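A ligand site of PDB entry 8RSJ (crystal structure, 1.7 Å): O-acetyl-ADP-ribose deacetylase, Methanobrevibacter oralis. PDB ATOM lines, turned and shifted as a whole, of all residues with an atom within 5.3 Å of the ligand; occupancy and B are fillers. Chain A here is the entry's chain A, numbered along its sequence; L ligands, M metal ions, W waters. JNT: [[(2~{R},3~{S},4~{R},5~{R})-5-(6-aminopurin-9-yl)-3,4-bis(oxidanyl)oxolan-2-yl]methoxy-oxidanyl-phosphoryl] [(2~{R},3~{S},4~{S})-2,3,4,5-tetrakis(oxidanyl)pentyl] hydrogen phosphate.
Water W9 lies within hydrogen-bond range of O4C of the ligand, O of Ala 101 and N of Asp 118. Water W10 lies within hydrogen-bond range of O3' of the ligand, N of Phe 247, OD2 of Asp 251, N of Thr 248 and SG of Cys 207. Water W1 lies within hydrogen-bond range of OG1 of Thr 210 (2.7 Å), O3' of the ligand (2.7 Å) and OD2 of Asp 251 (2.9 Å). Water W5 lies within hydrogen-bond range of the backbone carbonyl oxygen (O) of Ala 102 and an oxygen (O3C) of the ligand. Water W2 lies within hydrogen-bond range of O of Asn 115 (2.8 Å) and N7 of the ligand (2.9 Å). Water W3 lies within hydrogen-bond range of O of Asp 245, N of Cys 207 and N3 of the ligand.
The side-chain sulfur of Cys 116 sits close to the backbone NH of Asp 118, at 3.8 Å. The side-chain carboxylate (OD2) of Asp 118 is in hydrogen-bond range of the side-chain amide nitrogen (ND2) of Asn 103, 3.5 Å away. The side-chain carboxylate (OD1) of Asp 89 lies within hydrogen-bond range of the side-chain hydroxyl (OG1) of Thr 91 (2.7 Å). The side-chain amide nitrogen of Asn 103 lies within hydrogen-bond range of the backbone carbonyl oxygen of Gly 108 (2.9 Å). The backbone carbonyl oxygen (O) of Gly 88 sits close to the side-chain carboxylate (OD1) of Asp 245. The side-chain hydroxyl (OG1) of Thr 210 is in hydrogen-bond range of the backbone carbonyl oxygen (O) of Cys 207. The backbone NH of Ile 90 lies close to the side-chain carboxylate of Asp 245, at 3.4 Å. N of Gly 88 is in hydrogen-bond range of O of Val 246 (3.1 Å).
The backbone NH (N) of Ile 90 is in hydrogen-bond range of a nitrogen (N1) of the ligand (3.0 Å). The backbone NH (N) of Thr 210 sits at hydrogen-bond distance from an oxygen (O2B) of the ligand (3.5 Å). An oxygen (O1C) of the ligand is in hydrogen-bond range of the side-chain amide nitrogen (ND2) of Asn 103, 2.9 Å away. OD1 of Asp 89 is in hydrogen-bond range of N6 of the ligand. O2B of the ligand is in hydrogen-bond range of N of Gly 211 (2.7 Å). O1A of the ligand sits at hydrogen-bond distance from N of Ile 117, at 2.8 Å. The backbone NH (N) of Phe 213 sits at hydrogen-bond distance from an oxygen (O2B) of the ligand, 3.0 Å away. The side-chain carboxylate of Asp 118 sits at hydrogen-bond distance from an oxygen (O1C) of the ligand (2.6 Å). An oxygen (O1B) of the ligand sits at hydrogen-bond distance from the backbone NH (N) of Ser 209 (2.7 Å). The side-chain hydroxyl of Thr 210 lies within hydrogen-bond range of an oxygen (O3') of the ligand, 3.3 Å away. O3C of the ligand lies within hydrogen-bond range of O of Ala 102. The backbone NH (N) of Val 212 sits at hydrogen-bond distance from an oxygen (O2A) of the ligand, 3.0 Å away.
Residues that only touch the ligand: Gly 88 (3.6 Å), Ala 101 (3.5 Å), Cys 109 (3.9 Å), Cys 116 (3.6 Å), Ile 120 (3.8 Å), Cys 206 (3.9 Å), Cys 207 (3.3 Å), Ile 208 (3.8 Å), Asp 245 (3.8 Å) and Phe 247 (3.4 Å). Hydrophobic or aromatic side chains within 4 Å of the ligand: Ile 90, Ala 101, Ile 117, Ile 120, Val 212, Phe 213 and Phe 247. The nearest printed residue that does not touch the ligand is Asp 251 (4.1 Å).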
ATOM      1  N   GLY A  88      36.355  -0.054 -22.336  1.00  0.00           N
ATOM      2  CA  GLY A  88      35.753  -1.183 -23.000  1.00  0.00           C
ATOM      3  C   GLY A  88      34.349  -1.435 -22.505  1.00  0.00           C
ATOM      4  O   GLY A  88      33.771  -0.607 -21.806  1.00  0.00           O
ATOM      5  N   ASP A  89      33.820  -2.595 -22.903  1.00  0.00           N
ATOM      6  CA  ASP A  89      32.431  -2.956 -22.670  1.00  0.00           C
ATOM      7  C   ASP A  89      32.329  -3.573 -21.273  1.00  0.00           C
ATOM      8  O   ASP A  89      32.960  -4.601 -21.011  1.00  0.00           O
ATOM      9  CB  ASP A  89      31.966  -3.865 -23.828  1.00  0.00           C
ATOM     10  CG  ASP A  89      30.635  -4.579 -23.673  1.00  0.00           C
ATOM     11  OD1 ASP A  89      29.934  -4.355 -22.660  1.00  0.00           O
ATOM     12  OD2 ASP A  89      30.334  -5.403 -24.551  1.00  0.00           O
ATOM     13  N   ILE A  90      31.443  -3.007 -20.435  1.00  0.00           N
ATOM     14  CA  ILE A  90      31.350  -3.388 -19.030  1.00  0.00           C
ATOM     15  C   ILE A  90      30.848  -4.832 -18.894  1.00  0.00           C
ATOM     16  O   ILE A  90      31.120  -5.463 -17.861  1.00  0.00           O
ATOM     17  CB  ILE A  90      30.482  -2.373 -18.243  1.00  0.00           C
ATOM     18  CG1 ILE A  90      30.727  -2.447 -16.731  1.00  0.00           C
ATOM     19  CG2 ILE A  90      29.016  -2.568 -18.563  1.00  0.00           C
ATOM     20  CD1 ILE A  90      30.282  -1.230 -15.940  1.00  0.00           C
ATOM     21  N   THR A  91      30.116  -5.364 -19.902  1.00  0.00           N
ATOM     22  CA  THR A  91      29.637  -6.735 -19.851  1.00  0.00           C
ATOM     23  C   THR A  91      30.733  -7.776 -20.124  1.00  0.00           C
ATOM     24  O   THR A  91      30.411  -8.964 -20.112  1.00  0.00           O
ATOM     25  CB  THR A  91      28.428  -6.958 -20.779  1.00  0.00           C
ATOM     26  OG1 THR A  91      28.814  -6.739 -22.138  1.00  0.00           O
ATOM     27  CG2 THR A  91      27.284  -6.037 -20.398  1.00  0.00           C
ATOM     28  N   ALA A 101      23.688   2.262 -14.803  1.00  0.00           N
ATOM     29  CA  ALA A 101      22.895   3.484 -14.813  1.00  0.00           C
ATOM     30  C   ALA A 101      21.446   3.119 -15.149  1.00  0.00           C
ATOM     31  O   ALA A 101      21.013   3.085 -16.289  1.00  0.00           O
ATOM     32  CB  ALA A 101      23.455   4.485 -15.768  1.00  0.00           C
ATOM     33  N   ALA A 102      20.700   2.797 -14.097  1.00  0.00           N
ATOM     34  CA  ALA A 102      19.354   2.260 -14.191  1.00  0.00           C
ATOM     35  C   ALA A 102      18.345   3.383 -14.245  1.00  0.00           C
ATOM     36  O   ALA A 102      18.716   4.543 -14.007  1.00  0.00           O
ATOM     37  CB  ALA A 102      19.035   1.376 -13.019  1.00  0.00           C
ATOM     38  N   ASN A 103      17.094   3.058 -14.599  1.00  0.00           N
ATOM     39  CA  ASN A 103      16.025   4.068 -14.501  1.00  0.00           C
ATOM     40  C   ASN A 103      15.329   3.897 -13.157  1.00  0.00           C
ATOM     41  O   ASN A 103      15.498   2.835 -12.530  1.00  0.00           O
ATOM     42  CB  ASN A 103      15.053   4.103 -15.688  1.00  0.00           C
ATOM     43  CG  ASN A 103      14.387   2.779 -15.963  1.00  0.00           C
ATOM     44  OD1 ASN A 103      13.642   2.322 -15.111  1.00  0.00           O
ATOM     45  ND2 ASN A 103      14.678   2.157 -17.090  1.00  0.00           N
ATOM     46  N   GLY A 108      15.141  -2.341 -15.794  1.00  0.00           N
ATOM     47  CA  GLY A 108      15.851  -2.355 -17.045  1.00  0.00           C
ATOM     48  C   GLY A 108      15.094  -1.563 -18.117  1.00  0.00           C
ATOM     49  O   GLY A 108      14.299  -0.669 -17.841  1.00  0.00           O
ATOM     50  N   CYS A 109      15.446  -1.897 -19.367  1.00  0.00           N
ATOM     51  CA  CYS A 109      14.991  -1.111 -20.501  1.00  0.00           C
ATOM     52  C   CYS A 109      14.074  -1.987 -21.339  1.00  0.00           C
ATOM     53  O   CYS A 109      14.462  -3.072 -21.757  1.00  0.00           O
ATOM     54  CB  CYS A 109      16.218  -0.723 -21.299  1.00  0.00           C
ATOM     55  SG  CYS A 109      15.804   0.078 -22.858  1.00  0.00           S
ATOM     56  N   ASN A 115      20.593   0.792 -27.073  1.00  0.00           N
ATOM     57  CA  ASN A 115      21.966   0.585 -26.637  1.00  0.00           C
ATOM     58  C   ASN A 115      22.342   1.470 -25.450  1.00  0.00           C
ATOM     59  O   ASN A 115      23.530   1.719 -25.220  1.00  0.00           O
ATOM     60  CB  ASN A 115      22.952   0.585 -27.814  1.00  0.00           C
ATOM     61  CG  ASN A 115      22.796  -0.587 -28.778  1.00  0.00           C
ATOM     62  OD1 ASN A 115      22.777  -1.767 -28.405  1.00  0.00           O
ATOM     63  ND2 ASN A 115      22.756  -0.281 -30.068  1.00  0.00           N
ATOM     64  N   CYS A 116      21.358   1.785 -24.563  1.00  0.00           N
ATOM     65  CA  CYS A 116      21.699   2.291 -23.236  1.00  0.00           C
ATOM     66  C   CYS A 116      22.429   1.174 -22.455  1.00  0.00           C
ATOM     67  O   CYS A 116      22.269  -0.048 -22.706  1.00  0.00           O
ATOM     68  CB  CYS A 116      20.438   2.784 -22.520  1.00  0.00           C
ATOM     69  SG  CYS A 116      19.385   1.369 -22.065  1.00  0.00           S
ATOM     70  N   ILE A 117      23.253   1.549 -21.465  1.00  0.00           N
ATOM     71  CA  ILE A 117      24.005   0.538 -20.713  1.00  0.00           C
ATOM     72  C   ILE A 117      23.054  -0.374 -19.930  1.00  0.00           C
ATOM     73  O   ILE A 117      23.334  -1.542 -19.706  1.00  0.00           O
ATOM     74  CB  ILE A 117      25.078   1.157 -19.797  1.00  0.00           C
ATOM     75  CG1 ILE A 117      26.207   0.137 -19.583  1.00  0.00           C
ATOM     76  CG2 ILE A 117      24.478   1.715 -18.473  1.00  0.00           C
ATOM     77  CD1 ILE A 117      27.313   0.648 -18.749  1.00  0.00           C
ATOM     78  N   ASP A 118      21.866   0.148 -19.522  1.00  0.00           N
ATOM     79  CA  ASP A 118      20.863  -0.625 -18.780  1.00  0.00           C
ATOM     80  C   ASP A 118      20.379  -1.834 -19.609  1.00  0.00           C
ATOM     81  O   ASP A 118      20.346  -2.966 -19.111  1.00  0.00           O
ATOM     82  CB  ASP A 118      19.762   0.356 -18.382  1.00  0.00           C
ATOM     83  CG  ASP A 118      18.688  -0.184 -17.453  1.00  0.00           C
ATOM     84  OD1 ASP A 118      18.939  -1.135 -16.744  1.00  0.00           O
ATOM     85  OD2 ASP A 118      17.586   0.303 -17.518  1.00  0.00           O
ATOM     86  N   ILE A 120      21.876  -3.124 -22.224  1.00  0.00           N
ATOM     87  CA  ILE A 120      23.014  -3.977 -22.509  1.00  0.00           C
ATOM     88  C   ILE A 120      23.335  -4.904 -21.336  1.00  0.00           C
ATOM     89  O   ILE A 120      23.614  -6.108 -21.527  1.00  0.00           O
ATOM     90  CB  ILE A 120      24.191  -3.098 -22.934  1.00  0.00           C
ATOM     91  CG1 ILE A 120      23.815  -2.548 -24.314  1.00  0.00           C
ATOM     92  CG2 ILE A 120      25.521  -3.840 -22.888  1.00  0.00           C
ATOM     93  CD1 ILE A 120      24.834  -1.752 -24.988  1.00  0.00           C
ATOM     94  N   CYS A 206      30.444   2.742 -14.783  1.00  0.00           N
ATOM     95  CA  CYS A 206      30.232   3.436 -16.039  1.00  0.00           C
ATOM     96  C   CYS A 206      30.212   4.947 -15.802  1.00  0.00           C
ATOM     97  O   CYS A 206      30.105   5.395 -14.664  1.00  0.00           O
ATOM     98  CB  CYS A 206      28.964   2.999 -16.744  1.00  0.00           C
ATOM     99  SG  CYS A 206      27.452   3.314 -15.767  1.00  0.00           S
ATOM    100  N   CYS A 207      30.276   5.710 -16.898  1.00  0.00           N
ATOM    101  CA  CYS A 207      30.230   7.163 -16.843  1.00  0.00           C
ATOM    102  C   CYS A 207      28.779   7.632 -16.608  1.00  0.00           C
ATOM    103  O   CYS A 207      28.158   8.148 -17.508  1.00  0.00           O
ATOM    104  CB  CYS A 207      30.790   7.789 -18.101  1.00  0.00           C
ATOM    105  SG  CYS A 207      32.553   7.465 -18.315  1.00  0.00           S
ATOM    106  N   ILE A 208      28.264   7.428 -15.383  1.00  0.00           N
ATOM    107  CA  ILE A 208      26.894   7.720 -14.988  1.00  0.00           C
ATOM    108  C   ILE A 208      26.449   9.078 -15.497  1.00  0.00           C
ATOM    109  O   ILE A 208      27.120  10.077 -15.222  1.00  0.00           O
ATOM    110  CB  ILE A 208      26.743   7.574 -13.449  1.00  0.00           C
ATOM    111  CG1 ILE A 208      27.064   6.156 -12.943  1.00  0.00           C
ATOM    112  CG2 ILE A 208      25.382   8.016 -12.971  1.00  0.00           C
ATOM    113  CD1 ILE A 208      27.304   6.113 -11.442  1.00  0.00           C
ATOM    114  N   SER A 209      25.261   9.151 -16.131  1.00  0.00           N
ATOM    115  CA  SER A 209      24.558  10.378 -16.442  1.00  0.00           C
ATOM    116  C   SER A 209      25.138  11.096 -17.657  1.00  0.00           C
ATOM    117  O   SER A 209      24.515  12.084 -18.048  1.00  0.00           O
ATOM    118  CB  SER A 209      24.351  11.276 -15.267  1.00  0.00           C
ATOM    119  OG  SER A 209      23.397  10.666 -14.372  1.00  0.00           O
ATOM    120  N   THR A 210      26.240  10.609 -18.265  1.00  0.00           N
ATOM    121  CA  THR A 210      26.880  11.324 -19.359  1.00  0.00           C
ATOM    122  C   THR A 210      26.465  10.800 -20.733  1.00  0.00           C
ATOM    123  O   THR A 210      26.923  11.356 -21.713  1.00  0.00           O
ATOM    124  CB  THR A 210      28.407  11.232 -19.282  1.00  0.00           C
ATOM    125  OG1 THR A 210      28.780   9.870 -19.566  1.00  0.00           O
ATOM    126  CG2 THR A 210      28.869  11.761 -17.947  1.00  0.00           C
ATOM    127  N   GLY A 211      25.675   9.712 -20.784  1.00  0.00           N
ATOM    128  CA  GLY A 211      25.104   9.273 -22.047  1.00  0.00           C
ATOM    129  C   GLY A 211      23.886  10.139 -22.419  1.00  0.00           C
ATOM    130  O   GLY A 211      23.993  11.369 -22.576  1.00  0.00           O
ATOM    131  N   VAL A 212      22.707   9.480 -22.468  1.00  0.00           N
ATOM    132  CA  VAL A 212      21.451  10.141 -22.777  1.00  0.00           C
ATOM    133  C   VAL A 212      21.125  11.181 -21.721  1.00  0.00           C
ATOM    134  O   VAL A 212      20.333  12.062 -21.979  1.00  0.00           O
ATOM    135  CB  VAL A 212      20.292   9.132 -22.959  1.00  0.00           C
ATOM    136  CG1 VAL A 212      19.872   8.437 -21.667  1.00  0.00           C
ATOM    137  CG2 VAL A 212      19.067   9.765 -23.616  1.00  0.00           C
ATOM    138  N   PHE A 213      21.647  11.048 -20.476  1.00  0.00           N
ATOM    139  CA  PHE A 213      21.290  12.012 -19.432  1.00  0.00           C
ATOM    140  C   PHE A 213      22.053  13.336 -19.553  1.00  0.00           C
ATOM    141  O   PHE A 213      21.828  14.236 -18.761  1.00  0.00           O
ATOM    142  CB  PHE A 213      21.379  11.383 -18.043  1.00  0.00           C
ATOM    143  CG  PHE A 213      20.106  10.762 -17.561  1.00  0.00           C
ATOM    144  CD1 PHE A 213      18.983  10.577 -18.366  1.00  0.00           C
ATOM    145  CD2 PHE A 213      20.022  10.400 -16.223  1.00  0.00           C
ATOM    146  CE1 PHE A 213      17.827  10.025 -17.846  1.00  0.00           C
ATOM    147  CE2 PHE A 213      18.855   9.859 -15.721  1.00  0.00           C
ATOM    148  CZ  PHE A 213      17.750   9.701 -16.521  1.00  0.00           C
ATOM    149  N   ASN A 214      22.951  13.464 -20.520  1.00  0.00           N
ATOM    150  CA  ASN A 214      23.485  14.785 -20.920  1.00  0.00           C
ATOM    151  C   ASN A 214      24.295  15.483 -19.811  1.00  0.00           C
ATOM    152  O   ASN A 214      24.592  16.692 -19.928  1.00  0.00           O
ATOM    153  CB  ASN A 214      22.335  15.661 -21.429  1.00  0.00           C
ATOM    154  CG  ASN A 214      22.737  16.920 -22.169  1.00  0.00           C
ATOM    155  OD1 ASN A 214      23.545  16.850 -23.099  1.00  0.00           O
ATOM    156  ND2 ASN A 214      22.190  18.060 -21.788  1.00  0.00           N
ATOM    157  N   ASP A 245      35.421   2.486 -16.000  1.00  0.00           N
ATOM    158  CA  ASP A 245      35.133   1.892 -17.288  1.00  0.00           C
ATOM    159  C   ASP A 245      34.539   2.964 -18.201  1.00  0.00           C
ATOM    160  O   ASP A 245      33.374   3.310 -18.047  1.00  0.00           O
ATOM    161  CB  ASP A 245      34.245   0.654 -17.109  1.00  0.00           C
ATOM    162  CG  ASP A 245      33.892  -0.006 -18.419  1.00  0.00           C
ATOM    163  OD1 ASP A 245      34.309   0.494 -19.478  1.00  0.00           O
ATOM    164  OD2 ASP A 245      33.212  -1.018 -18.398  1.00  0.00           O
ATOM    165  N   VAL A 246      35.330   3.500 -19.133  1.00  0.00           N
ATOM    166  CA  VAL A 246      34.890   4.474 -20.122  1.00  0.00           C
ATOM    167  C   VAL A 246      34.512   3.762 -21.423  1.00  0.00           C
ATOM    168  O   VAL A 246      35.071   2.708 -21.729  1.00  0.00           O
ATOM    169  CB  VAL A 246      35.932   5.585 -20.382  1.00  0.00           C
ATOM    170  CG1 VAL A 246      36.140   6.477 -19.170  1.00  0.00           C
ATOM    171  CG2 VAL A 246      37.272   5.043 -20.855  1.00  0.00           C
ATOM    172  N   PHE A 247      33.577   4.346 -22.171  1.00  0.00           N
ATOM    173  CA  PHE A 247      33.067   3.729 -23.379  1.00  0.00           C
ATOM    174  C   PHE A 247      33.467   4.572 -24.610  1.00  0.00           C
ATOM    175  O   PHE A 247      33.722   3.979 -25.658  1.00  0.00           O
ATOM    176  CB  PHE A 247      31.571   3.494 -23.296  1.00  0.00           C
ATOM    177  CG  PHE A 247      31.063   2.385 -24.190  1.00  0.00           C
ATOM    178  CD1 PHE A 247      31.531   1.080 -24.036  1.00  0.00           C
ATOM    179  CD2 PHE A 247      30.134   2.633 -25.181  1.00  0.00           C
ATOM    180  CE1 PHE A 247      31.088   0.064 -24.864  1.00  0.00           C
ATOM    181  CE2 PHE A 247      29.649   1.603 -25.968  1.00  0.00           C
ATOM    182  CZ  PHE A 247      30.129   0.320 -25.813  1.00  0.00           C
ATOM    183  N   THR A 248      33.582   5.902 -24.503  1.00  0.00           N
ATOM    184  CA  THR A 248      34.002   6.750 -25.616  1.00  0.00           C
ATOM    185  C   THR A 248      35.480   7.120 -25.461  1.00  0.00           C
ATOM    186  O   THR A 248      36.041   7.160 -24.374  1.00  0.00           O
ATOM    187  CB  THR A 248      33.120   8.002 -25.690  1.00  0.00           C
ATOM    188  OG1 THR A 248      33.505   8.874 -24.625  1.00  0.00           O
ATOM    189  CG2 THR A 248      31.638   7.674 -25.612  1.00  0.00           C
ATOM    190  N   ASP A 251      35.642  10.308 -23.252  1.00  0.00           N
ATOM    191  CA  ASP A 251      35.707   9.990 -21.830  1.00  0.00           C
ATOM    192  C   ASP A 251      37.093   9.484 -21.446  1.00  0.00           C
ATOM    193  O   ASP A 251      37.632   9.945 -20.446  1.00  0.00           O
ATOM    194  CB  ASP A 251      34.573   9.061 -21.380  1.00  0.00           C
ATOM    195  CG  ASP A 251      33.202   9.729 -21.483  1.00  0.00           C
ATOM    196  OD1 ASP A 251      33.059  10.811 -20.903  1.00  0.00           O
ATOM    197  OD2 ASP A 251      32.360   9.215 -22.230  1.00  0.00           O
HETATM  198  O5' JNT L   1      25.227   6.038 -20.559  1.00  0.00           O
HETATM  199  C5' JNT L   1      25.932   5.823 -19.366  1.00  0.00           C
HETATM  200  C4' JNT L   1      27.452   5.611 -19.862  1.00  0.00           C
HETATM  201  O4' JNT L   1      27.560   4.206 -20.217  1.00  0.00           O
HETATM  202  C3' JNT L   1      27.916   6.449 -21.121  1.00  0.00           C
HETATM  203  O3' JNT L   1      29.267   6.888 -20.887  1.00  0.00           O
HETATM  204  C2' JNT L   1      27.857   5.336 -22.179  1.00  0.00           C
HETATM  205  O2' JNT L   1      28.700   5.569 -23.311  1.00  0.00           O
HETATM  206  C1' JNT L   1      28.404   4.218 -21.475  1.00  0.00           C
HETATM  207  N9  JNT L   1      28.098   2.883 -22.047  1.00  0.00           N
HETATM  208  C8  JNT L   1      27.175   2.431 -22.922  1.00  0.00           C
HETATM  209  N7  JNT L   1      27.368   1.107 -23.109  1.00  0.00           N
HETATM  210  C5  JNT L   1      28.397   0.742 -22.353  1.00  0.00           C
HETATM  211  C4  JNT L   1      28.842   1.849 -21.699  1.00  0.00           C
HETATM  212  N3  JNT L   1      29.903   1.776 -20.857  1.00  0.00           N
HETATM  213  C2  JNT L   1      30.541   0.565 -20.658  1.00  0.00           C
HETATM  214  N1  JNT L   1      30.114  -0.519 -21.320  1.00  0.00           N
HETATM  215  C6  JNT L   1      29.059  -0.454 -22.159  1.00  0.00           C
HETATM  216  N6  JNT L   1      28.623  -1.604 -22.776  1.00  0.00           N
HETATM  217  O1C JNT L   1      16.875   2.331 -18.999  1.00  0.00           O
HETATM  218  C1A JNT L   1      17.756   3.145 -18.618  1.00  0.00           C
HETATM  219  C2A JNT L   1      17.483   4.617 -18.289  1.00  0.00           C
HETATM  220  O2C JNT L   1      16.601   5.217 -19.020  1.00  0.00           O
HETATM  221  C3A JNT L   1      18.586   5.493 -17.702  1.00  0.00           C
HETATM  222  O3C JNT L   1      17.863   6.340 -16.742  1.00  0.00           O
HETATM  223  C4A JNT L   1      19.460   6.312 -18.738  1.00  0.00           C
HETATM  224  O4C JNT L   1      20.147   5.414 -19.734  1.00  0.00           O
HETATM  225  C5A JNT L   1      20.439   7.056 -17.823  1.00  0.00           C
HETATM  226  O5A JNT L   1      21.308   7.903 -18.667  1.00  0.00           O
HETATM  227  PB  JNT L   1      22.874   7.651 -18.586  1.00  0.00           P
HETATM  228  O2B JNT L   1      23.491   8.849 -19.452  1.00  0.00           O
HETATM  229  O1B JNT L   1      23.329   7.655 -17.219  1.00  0.00           O
HETATM  230  O3A JNT L   1      23.118   6.219 -19.275  1.00  0.00           O
HETATM  231  PA  JNT L   1      23.626   5.759 -20.717  1.00  0.00           P
HETATM  232  O1A JNT L   1      23.365   4.242 -20.649  1.00  0.00           O
HETATM  233  O2A JNT L   1      23.033   6.578 -21.812  1.00  0.00           O
HETATM  234 ZN    ZN M   1      17.329   1.884 -22.910  1.00  0.00          ZN
HETATM  235  O   HOH W   1      29.498   9.288 -22.102  1.00  0.00           O
HETATM  236  O   HOH W   2      26.121   0.673 -25.642  1.00  0.00           O
HETATM  237  O   HOH W   3      31.085   4.113 -19.265  1.00  0.00           O
HETATM  238  O   HOH W   4      27.701  -2.118 -25.695  1.00  0.00           O
HETATM  239  O   HOH W   5      19.546   6.897 -14.553  1.00  0.00           O
HETATM  240  O   HOH W   6      16.643   3.211 -21.600  1.00  0.00           O
HETATM  241  O   HOH W   7      24.855   3.832 -24.739  1.00  0.00           O
HETATM  242  O   HOH W   8      22.162   7.996 -14.890  1.00  0.00           O
HETATM  243  O   HOH W   9      21.377   3.407 -19.009  1.00  0.00           O
HETATM  244  O   HOH W  10      31.727   6.433 -21.667  1.00  0.00           O
HETATM  245  O   HOH W  11      27.609   7.476 -25.002  1.00  0.00           O
